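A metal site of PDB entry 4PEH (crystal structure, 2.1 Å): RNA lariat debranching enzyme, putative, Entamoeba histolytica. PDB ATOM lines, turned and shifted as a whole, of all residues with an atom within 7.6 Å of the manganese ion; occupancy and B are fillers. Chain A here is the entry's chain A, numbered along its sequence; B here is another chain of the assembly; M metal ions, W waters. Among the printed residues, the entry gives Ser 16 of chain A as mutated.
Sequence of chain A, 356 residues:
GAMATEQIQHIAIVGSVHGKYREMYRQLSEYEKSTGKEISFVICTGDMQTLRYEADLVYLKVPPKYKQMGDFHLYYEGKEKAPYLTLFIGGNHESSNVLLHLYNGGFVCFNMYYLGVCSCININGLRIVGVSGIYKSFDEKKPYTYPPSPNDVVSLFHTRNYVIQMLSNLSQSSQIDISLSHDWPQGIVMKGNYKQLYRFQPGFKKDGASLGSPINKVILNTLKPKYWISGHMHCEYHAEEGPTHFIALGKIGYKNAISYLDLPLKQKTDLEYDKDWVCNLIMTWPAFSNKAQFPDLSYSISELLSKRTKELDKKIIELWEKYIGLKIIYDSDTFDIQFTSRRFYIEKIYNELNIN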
ATOM      1  N   SER A  16     -21.731  10.586  -7.936  1.00  0.00           N
ATOM      2  CA  SER A  16     -20.347  10.138  -8.049  1.00  0.00           C
ATOM      3  C   SER A  16     -20.148   8.724  -7.473  1.00  0.00           C
ATOM      4  O   SER A  16     -20.468   8.475  -6.317  1.00  0.00           O
ATOM      5  CB  SER A  16     -19.452  11.111  -7.288  1.00  0.00           C
ATOM      6  OG  SER A  16     -19.653  12.455  -7.719  1.00  0.00           O
ATOM      7  N   HIS A  18     -17.041   7.027  -7.441  1.00  0.00           N
ATOM      8  CA  HIS A  18     -15.703   6.950  -6.850  1.00  0.00           C
ATOM      9  C   HIS A  18     -15.217   5.510  -6.731  1.00  0.00           C
ATOM     10  O   HIS A  18     -14.580   5.135  -5.738  1.00  0.00           O
ATOM     11  CB  HIS A  18     -15.667   7.633  -5.475  1.00  0.00           C
ATOM     12  CG  HIS A  18     -15.827   9.120  -5.525  1.00  0.00           C
ATOM     13  ND1 HIS A  18     -15.026   9.925  -6.304  1.00  0.00           N
ATOM     14  CD2 HIS A  18     -16.673   9.950  -4.884  1.00  0.00           C
ATOM     15  CE1 HIS A  18     -15.386  11.192  -6.153  1.00  0.00           C
ATOM     16  NE2 HIS A  18     -16.389  11.231  -5.288  1.00  0.00           N
ATOM     17  N   THR A  45     -23.669   9.757 -13.148  1.00  0.00           N
ATOM     18  CA  THR A  45     -23.211  11.075 -13.577  1.00  0.00           C
ATOM     19  C   THR A  45     -21.720  11.383 -13.393  1.00  0.00           C
ATOM     20  O   THR A  45     -21.329  12.556 -13.429  1.00  0.00           O
ATOM     21  CB  THR A  45     -24.041  12.180 -12.896  1.00  0.00           C
ATOM     22  OG1 THR A  45     -23.972  12.027 -11.478  1.00  0.00           O
ATOM     23  CG2 THR A  45     -25.490  12.082 -13.332  1.00  0.00           C
ATOM     24  N   GLY A  46     -20.891  10.366 -13.211  1.00  0.00           N
ATOM     25  CA  GLY A  46     -19.446  10.583 -13.291  1.00  0.00           C
ATOM     26  C   GLY A  46     -18.597  10.156 -12.101  1.00  0.00           C
ATOM     27  O   GLY A  46     -19.125   9.690 -11.093  1.00  0.00           O
ATOM     28  N   ASP A  47     -17.283  10.354 -12.236  1.00  0.00           N
ATOM     29  CA  ASP A  47     -16.299   9.906 -11.249  1.00  0.00           C
ATOM     30  C   ASP A  47     -16.357   8.387 -11.098  1.00  0.00           C
ATOM     31  O   ASP A  47     -16.415   7.855  -9.983  1.00  0.00           O
ATOM     32  CB  ASP A  47     -16.453  10.631  -9.905  1.00  0.00           C
ATOM     33  CG  ASP A  47     -15.941  12.064  -9.960  1.00  0.00           C
ATOM     34  OD1 ASP A  47     -15.250  12.405 -10.932  1.00  0.00           O
ATOM     35  OD2 ASP A  47     -16.227  12.836  -9.005  1.00  0.00           O
ATOM     36  N   GLY A  91     -16.416  12.003 -15.203  1.00  0.00           N
ATOM     37  CA  GLY A  91     -16.349  13.127 -14.288  1.00  0.00           C
ATOM     38  C   GLY A  91     -14.946  13.708 -14.237  1.00  0.00           C
ATOM     39  O   GLY A  91     -14.280  13.803 -15.263  1.00  0.00           O
ATOM     40  N   ASN A  92     -14.494  14.092 -13.048  1.00  0.00           N
ATOM     41  CA  ASN A  92     -13.144  14.640 -12.901  1.00  0.00           C
ATOM     42  C   ASN A  92     -12.172  13.643 -12.274  1.00  0.00           C
ATOM     43  O   ASN A  92     -10.964  13.889 -12.220  1.00  0.00           O
ATOM     44  CB  ASN A  92     -13.160  15.949 -12.100  1.00  0.00           C
ATOM     45  CG  ASN A  92     -13.855  15.805 -10.758  1.00  0.00           C
ATOM     46  OD1 ASN A  92     -15.078  15.664 -10.683  1.00  0.00           O
ATOM     47  ND2 ASN A  92     -13.071  15.837  -9.676  1.00  0.00           N
ATOM     48  N   HIS A  93     -12.701  12.519 -11.796  1.00  0.00           N
ATOM     49  CA  HIS A  93     -11.880  11.431 -11.276  1.00  0.00           C
ATOM     50  C   HIS A  93     -12.104  10.170 -12.106  1.00  0.00           C
ATOM     51  O   HIS A  93     -13.047   9.419 -11.852  1.00  0.00           O
ATOM     52  CB  HIS A  93     -12.188  11.179  -9.794  1.00  0.00           C
ATOM     53  CG  HIS A  93     -11.915  12.345  -8.903  1.00  0.00           C
ATOM     54  ND1 HIS A  93     -10.725  13.043  -8.937  1.00  0.00           N
ATOM     55  CD2 HIS A  93     -12.680  12.934  -7.953  1.00  0.00           C
ATOM     56  CE1 HIS A  93     -10.772  14.022  -8.042  1.00  0.00           C
ATOM     57  NE2 HIS A  93     -11.939  13.975  -7.430  1.00  0.00           N
ATOM     58  N   GLU A  94     -11.259   9.942 -13.107  1.00  0.00           N
ATOM     59  CA  GLU A  94     -11.445   8.832 -14.035  1.00  0.00           C
ATOM     60  C   GLU A  94     -10.133   8.175 -14.420  1.00  0.00           C
ATOM     61  O   GLU A  94      -9.053   8.770 -14.262  1.00  0.00           O
ATOM     62  CB  GLU A  94     -12.117   9.326 -15.321  1.00  0.00           C
ATOM     63  CG  GLU A  94     -13.443  10.054 -15.118  1.00  0.00           C
ATOM     64  CD  GLU A  94     -14.565   9.136 -14.692  1.00  0.00           C
ATOM     65  OE1 GLU A  94     -14.373   7.905 -14.677  1.00  0.00           O
ATOM     66  OE2 GLU A  94     -15.649   9.651 -14.369  1.00  0.00           O
ATOM     67  N   ILE A 134     -15.494  18.132 -16.349  1.00  0.00           N
ATOM     68  CA  ILE A 134     -15.837  19.368 -15.654  1.00  0.00           C
ATOM     69  C   ILE A 134     -15.185  20.567 -16.354  1.00  0.00           C
ATOM     70  O   ILE A 134     -14.260  20.409 -17.149  1.00  0.00           O
ATOM     71  CB  ILE A 134     -15.417  19.367 -14.176  1.00  0.00           C
ATOM     72  CG1 ILE A 134     -13.893  19.278 -14.038  1.00  0.00           C
ATOM     73  CG2 ILE A 134     -16.121  18.247 -13.416  1.00  0.00           C
ATOM     74  CD1 ILE A 134     -13.405  19.493 -12.618  1.00  0.00           C
ATOM     75  N   HIS A 182     -21.410  16.099 -15.311  1.00  0.00           N
ATOM     76  CA  HIS A 182     -20.819  15.906 -13.986  1.00  0.00           C
ATOM     77  C   HIS A 182     -21.027  17.159 -13.141  1.00  0.00           C
ATOM     78  O   HIS A 182     -21.775  17.119 -12.158  1.00  0.00           O
ATOM     79  CB  HIS A 182     -19.345  15.499 -14.059  1.00  0.00           C
ATOM     80  CG  HIS A 182     -18.805  14.990 -12.764  1.00  0.00           C
ATOM     81  ND1 HIS A 182     -19.271  13.828 -12.178  1.00  0.00           N
ATOM     82  CD2 HIS A 182     -17.866  15.478 -11.926  1.00  0.00           C
ATOM     83  CE1 HIS A 182     -18.618  13.621 -11.048  1.00  0.00           C
ATOM     84  NE2 HIS A 182     -17.763  14.620 -10.866  1.00  0.00           N
ATOM     85  N   ASP A 183     -20.385  18.263 -13.508  1.00  0.00           N
ATOM     86  CA  ASP A 183     -20.609  19.520 -12.787  1.00  0.00           C
ATOM     87  C   ASP A 183     -21.926  20.182 -13.219  1.00  0.00           C
ATOM     88  O   ASP A 183     -22.432  19.913 -14.303  1.00  0.00           O
ATOM     89  CB  ASP A 183     -19.411  20.469 -12.890  1.00  0.00           C
ATOM     90  CG  ASP A 183     -18.981  20.736 -14.315  1.00  0.00           C
ATOM     91  OD1 ASP A 183     -19.454  20.039 -15.246  1.00  0.00           O
ATOM     92  OD2 ASP A 183     -18.140  21.642 -14.501  1.00  0.00           O
ATOM     93  N   GLY A 231     -23.891  15.246 -10.939  1.00  0.00           N
ATOM     94  CA  GLY A 231     -23.379  14.835  -9.648  1.00  0.00           C
ATOM     95  C   GLY A 231     -22.403  15.888  -9.183  1.00  0.00           C
ATOM     96  O   GLY A 231     -22.635  17.087  -9.339  1.00  0.00           O
ATOM     97  N   HIS A 232     -21.336  15.412  -8.564  1.00  0.00           N
ATOM     98  CA  HIS A 232     -20.075  16.152  -8.393  1.00  0.00           C
ATOM     99  C   HIS A 232     -20.026  16.952  -7.101  1.00  0.00           C
ATOM    100  O   HIS A 232     -18.996  16.986  -6.418  1.00  0.00           O
ATOM    101  CB  HIS A 232     -19.760  17.072  -9.583  1.00  0.00           C
ATOM    102  CG  HIS A 232     -18.479  17.832  -9.455  1.00  0.00           C
ATOM    103  ND1 HIS A 232     -17.265  17.213  -9.226  1.00  0.00           N
ATOM    104  CD2 HIS A 232     -18.214  19.162  -9.513  1.00  0.00           C
ATOM    105  CE1 HIS A 232     -16.309  18.122  -9.148  1.00  0.00           C
ATOM    106  NE2 HIS A 232     -16.865  19.313  -9.318  1.00  0.00           N
ATOM    107  N   MET A 233     -21.145  17.597  -6.756  1.00  0.00           N
ATOM    108  CA  MET A 233     -21.182  18.574  -5.661  1.00  0.00           C
ATOM    109  C   MET A 233     -21.445  17.986  -4.264  1.00  0.00           C
ATOM    110  O   MET A 233     -21.602  18.749  -3.299  1.00  0.00           O
ATOM    111  CB  MET A 233     -22.205  19.671  -5.957  1.00  0.00           C
ATOM    112  CG  MET A 233     -21.889  20.483  -7.197  1.00  0.00           C
ATOM    113  SD  MET A 233     -20.280  21.293  -7.140  1.00  0.00           S
ATOM    114  CE  MET A 233     -20.573  22.518  -5.882  1.00  0.00           C
ATOM    115  N   HIS A 234     -21.481  16.670  -4.155  1.00  0.00           N
ATOM    116  CA  HIS A 234     -21.654  15.986  -2.866  1.00  0.00           C
ATOM    117  C   HIS A 234     -22.898  16.434  -2.102  1.00  0.00           C
ATOM    118  O   HIS A 234     -22.851  16.585  -0.884  1.00  0.00           O
ATOM    119  CB  HIS A 234     -20.407  16.166  -1.990  1.00  0.00           C
ATOM    120  CG  HIS A 234     -19.134  15.708  -2.633  1.00  0.00           C
ATOM    121  ND1 HIS A 234     -17.933  16.348  -2.444  1.00  0.00           N
ATOM    122  CD2 HIS A 234     -18.887  14.682  -3.477  1.00  0.00           C
ATOM    123  CE1 HIS A 234     -16.993  15.739  -3.130  1.00  0.00           C
ATOM    124  NE2 HIS A 234     -17.545  14.723  -3.775  1.00  0.00           N
ATOM    125  O5'   A B   3     -15.971  21.757   0.823  1.00  0.00           O
ATOM    126  C5'   A B   3     -17.082  20.870   0.655  1.00  0.00           C
ATOM    127  C4'   A B   3     -16.851  19.969  -0.543  1.00  0.00           C
ATOM    128  O4'   A B   3     -17.424  20.583  -1.725  1.00  0.00           O
ATOM    129  C3'   A B   3     -15.380  19.689  -0.878  1.00  0.00           C
ATOM    130  O3'   A B   3     -15.229  18.381  -1.429  1.00  0.00           O
ATOM    131  C2'   A B   3     -15.074  20.763  -1.921  1.00  0.00           C
ATOM    132  O2'   A B   3     -14.029  20.403  -2.800  1.00  0.00           O
ATOM    133  C1'   A B   3     -16.400  20.823  -2.682  1.00  0.00           C
ATOM    134  N9    A B   3     -16.653  22.124  -3.301  1.00  0.00           N
ATOM    135  C8    A B   3     -16.811  23.342  -2.675  1.00  0.00           C
ATOM    136  N7    A B   3     -17.034  24.336  -3.499  1.00  0.00           N
ATOM    137  C5    A B   3     -17.016  23.737  -4.749  1.00  0.00           C
ATOM    138  C6    A B   3     -17.180  24.258  -6.044  1.00  0.00           C
ATOM    139  N6    A B   3     -17.413  25.541  -6.304  1.00  0.00           N
ATOM    140  N1    A B   3     -17.108  23.397  -7.079  1.00  0.00           N
ATOM    141  C2    A B   3     -16.881  22.100  -6.825  1.00  0.00           C
ATOM    142  N3    A B   3     -16.709  21.493  -5.650  1.00  0.00           N
ATOM    143  C4    A B   3     -16.780  22.377  -4.642  1.00  0.00           C
ATOM    144  P1  A2P B   4     -14.917  15.627  -6.266  1.00  0.00           P
ATOM    145  O1P A2P B   4     -14.808  15.642  -7.777  1.00  0.00           O
ATOM    146  O2P A2P B   4     -15.209  17.025  -5.770  1.00  0.00           O
ATOM    147  O3P A2P B   4     -16.004  14.686  -5.812  1.00  0.00           O
ATOM    148  P2  A2P B   4     -14.574  17.207  -0.536  1.00  0.00           P
ATOM    149  O5P A2P B   4     -15.642  16.218  -0.247  1.00  0.00           O
ATOM    150  O6P A2P B   4     -13.826  17.850   0.565  1.00  0.00           O
ATOM    151  O5' A2P B   4     -13.519  16.503  -1.509  1.00  0.00           O
ATOM    152  C5' A2P B   4     -12.213  17.035  -1.707  1.00  0.00           C
ATOM    153  C4' A2P B   4     -11.504  16.364  -2.878  1.00  0.00           C
ATOM    154  O4' A2P B   4     -11.550  14.921  -2.716  1.00  0.00           O
ATOM    155  C3' A2P B   4     -12.125  16.629  -4.243  1.00  0.00           C
ATOM    156  O3' A2P B   4     -11.104  16.533  -5.228  1.00  0.00           O
ATOM    157  C2' A2P B   4     -13.104  15.464  -4.352  1.00  0.00           C
ATOM    158  O2' A2P B   4     -13.502  15.135  -5.665  1.00  0.00           O
ATOM    159  C1' A2P B   4     -12.225  14.341  -3.820  1.00  0.00           C
ATOM    160  N9  A2P B   4     -12.890  13.117  -3.366  1.00  0.00           N
ATOM    161  C8  A2P B   4     -13.839  12.977  -2.389  1.00  0.00           C
ATOM    162  N7  A2P B   4     -14.229  11.736  -2.199  1.00  0.00           N
ATOM    163  C5  A2P B   4     -13.473  11.008  -3.115  1.00  0.00           C
ATOM    164  C6  A2P B   4     -13.410   9.625  -3.412  1.00  0.00           C
ATOM    165  N6  A2P B   4     -14.135   8.689  -2.794  1.00  0.00           N
ATOM    166  N1  A2P B   4     -12.552   9.235  -4.380  1.00  0.00           N
ATOM    167  C2  A2P B   4     -11.813  10.167  -5.001  1.00  0.00           C
ATOM    168  N3  A2P B   4     -11.782  11.480  -4.799  1.00  0.00           N
ATOM    169  C4  A2P B   4     -12.642  11.846  -3.836  1.00  0.00           C
ATOM    170  P     C B   5     -10.266  17.831  -5.662  1.00  0.00           P
ATOM    171  OP1   C B   5      -9.226  17.392  -6.627  1.00  0.00           O
ATOM    172  OP2   C B   5      -9.862  18.579  -4.447  1.00  0.00           O
ATOM    173  O5'   C B   5     -11.313  18.715  -6.476  1.00  0.00           O
ATOM    174  C5'   C B   5     -11.841  18.251  -7.722  1.00  0.00           C
ATOM    175  C4'   C B   5     -11.888  19.336  -8.764  1.00  0.00           C
ATOM    176  O4'   C B   5     -12.796  20.389  -8.348  1.00  0.00           O
ATOM    177  C3'   C B   5     -10.554  20.024  -9.080  1.00  0.00           C
ATOM    178  O3'   C B   5     -10.497  20.329 -10.462  1.00  0.00           O
ATOM    179  C2'   C B   5     -10.656  21.331  -8.287  1.00  0.00           C
ATOM    180  O2'   C B   5      -9.848  22.378  -8.794  1.00  0.00           O
ATOM    181  C1'   C B   5     -12.140  21.636  -8.433  1.00  0.00           C
ATOM    182  N1    C B   5     -12.671  22.531  -7.395  1.00  0.00           N
ATOM    183  C2    C B   5     -13.259  23.732  -7.813  1.00  0.00           C
ATOM    184  O2    C B   5     -13.314  23.965  -9.031  1.00  0.00           O
ATOM    185  N3    C B   5     -13.758  24.591  -6.892  1.00  0.00           N
ATOM    186  C4    C B   5     -13.666  24.281  -5.593  1.00  0.00           C
ATOM    187  N4    C B   5     -14.166  25.159  -4.708  1.00  0.00           N
ATOM    188  C5    C B   5     -13.069  23.065  -5.141  1.00  0.00           C
ATOM    189  C6    C B   5     -12.580  22.224  -6.064  1.00  0.00           C
HETATM  190 MN    MN M   1     -16.401  14.969  -9.178  1.00  0.00          MN
HETATM  191  O   HOH W   1     -17.851  14.518  -7.310  1.00  0.00           O
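The side-chain amide nitrogen of Asn 92 lies within hydrogen-bond range of a ring nitrogen (NE2) of His 93. OD1 of Asp 47 sits at hydrogen-bond distance from N of His 93. The backbone NH of His 18 sits at hydrogen-bond distance from the backbone carbonyl oxygen of Asp 47, 2.7 Å away. The backbone carbonyl oxygen of His 182 sits at hydrogen-bond distance from the backbone NH of Gly 231. A ring nitrogen (ND1) of His 182 sits at hydrogen-bond distance from the backbone carbonyl oxygen (O) of Thr 45, 2.7 Å away. NE2 of His 93 sits at hydrogen-bond distance from O2' of A2P 4 of chain B, at 2.6 Å. N1 of A2P 4 of chain B sits at hydrogen-bond distance from ND1 of His 18 (3.2 Å). O3P of A2P 4 of chain B sits at hydrogen-bond distance from a ring nitrogen (NE2) of His 234 (2.6 Å).
Of the 19 residues printed, 5 come within 4 Å of the manganese ion. Along chain A the residues within 4 Å of the manganese ion span positions 47 to 232. The nearest printed residue that does not touch the manganese ion is Ser 16 (4.4 Å).
OD1 of Asn 92 is bound to the manganese ion. OD2 of Asp 47 is bound to the manganese ion, 2.1 Å away. The manganese ion is bound by a ring nitrogen (NE2) of His 182, 2.2 Å away. O1P of A2P 4 of chain B is bound to the manganese ion, at 2.2 Å. The manganese ion is bound by ND1 of His 232, 2.4 Å away. The manganese ion is bound by water W1 (2.4 Å).
Water W1 bridges the side-chain hydroxyl (OG) of Ser 16 (2.8 Å) and the backbone carbonyl oxygen (O) of His 232 (2.9 Å).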
